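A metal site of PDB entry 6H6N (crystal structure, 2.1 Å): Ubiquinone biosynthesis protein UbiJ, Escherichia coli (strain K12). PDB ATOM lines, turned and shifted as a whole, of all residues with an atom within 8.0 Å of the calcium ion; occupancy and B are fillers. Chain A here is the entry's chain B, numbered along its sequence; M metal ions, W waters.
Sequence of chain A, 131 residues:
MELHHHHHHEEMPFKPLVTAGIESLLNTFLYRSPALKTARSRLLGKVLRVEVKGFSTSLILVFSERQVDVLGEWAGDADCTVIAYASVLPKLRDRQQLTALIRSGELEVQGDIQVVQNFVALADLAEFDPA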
ATOM      1  N   PHE A  29     -35.880   7.470  25.022  1.00  0.00           N
ATOM      2  CA  PHE A  29     -34.694   7.458  24.182  1.00  0.00           C
ATOM      3  C   PHE A  29     -33.774   6.249  24.386  1.00  0.00           C
ATOM      4  O   PHE A  29     -33.311   5.700  23.412  1.00  0.00           O
ATOM      5  CB  PHE A  29     -33.909   8.787  24.367  1.00  0.00           C
ATOM      6  CG  PHE A  29     -32.725   8.953  23.453  1.00  0.00           C
ATOM      7  CD1 PHE A  29     -32.875   8.934  22.074  1.00  0.00           C
ATOM      8  CD2 PHE A  29     -31.466   9.240  23.983  1.00  0.00           C
ATOM      9  CE1 PHE A  29     -31.779   9.111  21.240  1.00  0.00           C
ATOM     10  CE2 PHE A  29     -30.377   9.428  23.143  1.00  0.00           C
ATOM     11  CZ  PHE A  29     -30.524   9.351  21.771  1.00  0.00           C
ATOM     12  N   ARG A  93     -23.977  12.464  22.766  1.00  0.00           N
ATOM     13  CA  ARG A  93     -24.568  11.390  21.962  1.00  0.00           C
ATOM     14  C   ARG A  93     -23.497  10.878  20.966  1.00  0.00           C
ATOM     15  O   ARG A  93     -23.813  10.144  20.021  1.00  0.00           O
ATOM     16  CB  ARG A  93     -25.814  11.876  21.204  1.00  0.00           C
ATOM     17  CG  ARG A  93     -27.039  12.135  22.081  1.00  0.00           C
ATOM     18  CD  ARG A  93     -28.132  12.808  21.270  1.00  0.00           C
ATOM     19  NE  ARG A  93     -27.974  14.261  21.199  1.00  0.00           N
ATOM     20  CZ  ARG A  93     -28.439  15.026  20.213  1.00  0.00           C
ATOM     21  NH1 ARG A  93     -29.053  14.484  19.175  1.00  0.00           N
ATOM     22  NH2 ARG A  93     -28.278  16.337  20.254  1.00  0.00           N
ATOM     23  N   ASP A  94     -22.222  11.276  21.180  1.00  0.00           N
ATOM     24  CA  ASP A  94     -21.105  10.877  20.340  1.00  0.00           C
ATOM     25  C   ASP A  94     -19.900  10.457  21.175  1.00  0.00           C
ATOM     26  O   ASP A  94     -19.215  11.298  21.767  1.00  0.00           O
ATOM     27  CB  ASP A  94     -20.749  11.975  19.332  1.00  0.00           C
ATOM     28  CG  ASP A  94     -19.712  11.620  18.255  1.00  0.00           C
ATOM     29  OD1 ASP A  94     -19.432  10.404  18.080  1.00  0.00           O
ATOM     30  OD2 ASP A  94     -19.249  12.546  17.555  1.00  0.00           O
ATOM     31  N   ARG A  95     -19.653   9.136  21.198  1.00  0.00           N
ATOM     32  CA  ARG A  95     -18.558   8.477  21.904  1.00  0.00           C
ATOM     33  C   ARG A  95     -17.166   8.909  21.495  1.00  0.00           C
ATOM     34  O   ARG A  95     -16.262   8.913  22.330  1.00  0.00           O
ATOM     35  CB  ARG A  95     -18.658   6.938  21.777  1.00  0.00           C
ATOM     36  CG  ARG A  95     -18.344   6.271  23.108  1.00  0.00           C
ATOM     37  CD  ARG A  95     -17.564   4.984  23.071  1.00  0.00           C
ATOM     38  NE  ARG A  95     -17.378   4.510  24.447  1.00  0.00           N
ATOM     39  CZ  ARG A  95     -16.817   3.361  24.812  1.00  0.00           C
ATOM     40  NH1 ARG A  95     -16.726   3.031  26.085  1.00  0.00           N
ATOM     41  NH2 ARG A  95     -16.337   2.532  23.888  1.00  0.00           N
ATOM     42  N   VAL A 120     -22.424   7.761  27.373  1.00  0.00           N
ATOM     43  CA  VAL A 120     -22.218   8.371  26.052  1.00  0.00           C
ATOM     44  C   VAL A 120     -22.237   7.241  24.967  1.00  0.00           C
ATOM     45  O   VAL A 120     -22.885   7.405  23.961  1.00  0.00           O
ATOM     46  CB  VAL A 120     -20.923   9.229  26.019  1.00  0.00           C
ATOM     47  CG1 VAL A 120     -20.510   9.588  24.598  1.00  0.00           C
ATOM     48  CG2 VAL A 120     -21.102  10.507  26.828  1.00  0.00           C
ATOM     49  N   ALA A 121     -21.577   6.098  25.215  1.00  0.00           N
ATOM     50  CA  ALA A 121     -21.591   4.951  24.275  1.00  0.00           C
ATOM     51  C   ALA A 121     -23.052   4.439  24.084  1.00  0.00           C
ATOM     52  O   ALA A 121     -23.413   4.126  22.968  1.00  0.00           O
ATOM     53  CB  ALA A 121     -20.710   3.827  24.817  1.00  0.00           C
ATOM     54  N   LEU A 122     -23.865   4.400  25.170  1.00  0.00           N
ATOM     55  CA  LEU A 122     -25.281   3.983  25.138  1.00  0.00           C
ATOM     56  C   LEU A 122     -26.130   4.971  24.290  1.00  0.00           C
ATOM     57  O   LEU A 122     -26.857   4.537  23.399  1.00  0.00           O
ATOM     58  CB  LEU A 122     -25.854   3.841  26.562  1.00  0.00           C
ATOM     59  CG  LEU A 122     -27.402   3.642  26.683  1.00  0.00           C
ATOM     60  CD1 LEU A 122     -27.884   2.378  25.958  1.00  0.00           C
ATOM     61  CD2 LEU A 122     -27.868   3.656  28.122  1.00  0.00           C
ATOM     62  N   ALA A 123     -26.013   6.283  24.578  1.00  0.00           N
ATOM     63  CA  ALA A 123     -26.726   7.365  23.879  1.00  0.00           C
ATOM     64  C   ALA A 123     -26.385   7.371  22.417  1.00  0.00           C
ATOM     65  O   ALA A 123     -27.279   7.602  21.610  1.00  0.00           O
ATOM     66  CB  ALA A 123     -26.423   8.713  24.505  1.00  0.00           C
ATOM     67  N   ASP A 124     -25.110   7.085  22.073  1.00  0.00           N
ATOM     68  CA  ASP A 124     -24.643   6.999  20.691  1.00  0.00           C
ATOM     69  C   ASP A 124     -25.291   5.805  19.969  1.00  0.00           C
ATOM     70  O   ASP A 124     -25.762   5.948  18.860  1.00  0.00           O
ATOM     71  CB  ASP A 124     -23.104   6.917  20.631  1.00  0.00           C
ATOM     72  CG  ASP A 124     -22.503   7.194  19.265  1.00  0.00           C
ATOM     73  OD1 ASP A 124     -23.263   7.475  18.312  1.00  0.00           O
ATOM     74  OD2 ASP A 124     -21.272   7.184  19.158  1.00  0.00           O
ATOM     75  N   LEU A 125     -25.354   4.654  20.639  1.00  0.00           N
ATOM     76  CA  LEU A 125     -26.017   3.472  20.057  1.00  0.00           C
ATOM     77  C   LEU A 125     -27.557   3.643  20.002  1.00  0.00           C
ATOM     78  O   LEU A 125     -28.205   3.008  19.190  1.00  0.00           O
ATOM     79  CB  LEU A 125     -25.664   2.217  20.846  1.00  0.00           C
ATOM     80  CG  LEU A 125     -24.239   1.723  20.680  1.00  0.00           C
ATOM     81  CD1 LEU A 125     -23.879   0.742  21.768  1.00  0.00           C
ATOM     82  CD2 LEU A 125     -23.989   1.170  19.265  1.00  0.00           C
ATOM     83  N   ALA A 126     -28.122   4.521  20.858  1.00  0.00           N
ATOM     84  CA  ALA A 126     -29.572   4.786  20.880  1.00  0.00           C
ATOM     85  C   ALA A 126     -30.031   5.580  19.664  1.00  0.00           C
ATOM     86  O   ALA A 126     -31.206   5.551  19.318  1.00  0.00           O
ATOM     87  CB  ALA A 126     -29.941   5.527  22.150  1.00  0.00           C
ATOM     88  N   GLU A 127     -29.116   6.293  18.999  1.00  0.00           N
ATOM     89  CA  GLU A 127     -29.542   7.172  17.917  1.00  0.00           C
ATOM     90  C   GLU A 127     -28.800   6.978  16.623  1.00  0.00           C
ATOM     91  O   GLU A 127     -27.574   6.824  16.618  1.00  0.00           O
ATOM     92  CB  GLU A 127     -29.409   8.610  18.447  1.00  0.00           C
ATOM     93  CG  GLU A 127     -29.448   9.758  17.457  1.00  0.00           C
ATOM     94  CD  GLU A 127     -28.940  11.029  18.105  1.00  0.00           C
ATOM     95  OE1 GLU A 127     -29.775  11.875  18.479  1.00  0.00           O
ATOM     96  OE2 GLU A 127     -27.718  11.135  18.326  1.00  0.00           O
ATOM     97  N   PHE A 128     -29.553   7.024  15.510  1.00  0.00           N
ATOM     98  CA  PHE A 128     -29.031   6.963  14.143  1.00  0.00           C
ATOM     99  C   PHE A 128     -28.399   8.327  13.831  1.00  0.00           C
ATOM    100  O   PHE A 128     -28.981   9.340  14.166  1.00  0.00           O
ATOM    101  CB  PHE A 128     -30.174   6.697  13.149  1.00  0.00           C
ATOM    102  CG  PHE A 128     -30.580   5.260  12.978  1.00  0.00           C
ATOM    103  CD1 PHE A 128     -29.824   4.392  12.195  1.00  0.00           C
ATOM    104  CD2 PHE A 128     -31.733   4.764  13.598  1.00  0.00           C
ATOM    105  CE1 PHE A 128     -30.214   3.055  12.022  1.00  0.00           C
ATOM    106  CE2 PHE A 128     -32.122   3.427  13.425  1.00  0.00           C
ATOM    107  CZ  PHE A 128     -31.358   2.582  12.641  1.00  0.00           C
ATOM    108  N   ASP A 129     -27.211   8.337  13.243  1.00  0.00           N
ATOM    109  CA  ASP A 129     -26.508   9.582  12.892  1.00  0.00           C
ATOM    110  C   ASP A 129     -27.025  10.131  11.562  1.00  0.00           C
ATOM    111  O   ASP A 129     -27.367   9.366  10.661  1.00  0.00           O
ATOM    112  CB  ASP A 129     -24.981   9.364  12.828  1.00  0.00           C
ATOM    113  CG  ASP A 129     -24.335   9.050  14.163  1.00  0.00           C
ATOM    114  OD1 ASP A 129     -24.860   8.182  14.895  1.00  0.00           O
ATOM    115  OD2 ASP A 129     -23.263   9.629  14.457  1.00  0.00           O
HETATM  116 CA    CA M   1     -25.354   7.406  17.182  1.00  0.00          CA
HETATM  117  O   HOH W   1     -25.672   9.363  18.011  1.00  0.00           O
HETATM  118  O   HOH W   2     -25.094   5.056  16.382  1.00  0.00           O
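Within 4 Å of the calcium ion: Asp 124, Glu 127 and Asp 129. The nearest printed residue that does not touch the calcium ion is Arg 93 (4.2 Å).
Water W1 binds the calcium ion. The calcium ion is bound by the backbone carbonyl oxygen (O) of Asp 124 (2.3 Å). O of Glu 127 is bound to the calcium ion, at 2.4 Å. OD1 of Asp 124 binds the calcium ion (2.4 Å). The side-chain carboxylate (OD1) of Asp 129 binds the calcium ion. Water W2 binds the calcium ion, 2.5 Å away.
Water W1 lies within hydrogen-bond range of OE2 of Glu 127 (2.7 Å) and O of Arg 93 (2.8 Å).
NH1 of Arg 93 lies within salt-bridge range of OE1 of Glu 127 (2.8 Å). The side-chain carboxylate of Asp 124 lies within hydrogen-bond range of the backbone NH of Arg 95 (3.3 Å).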
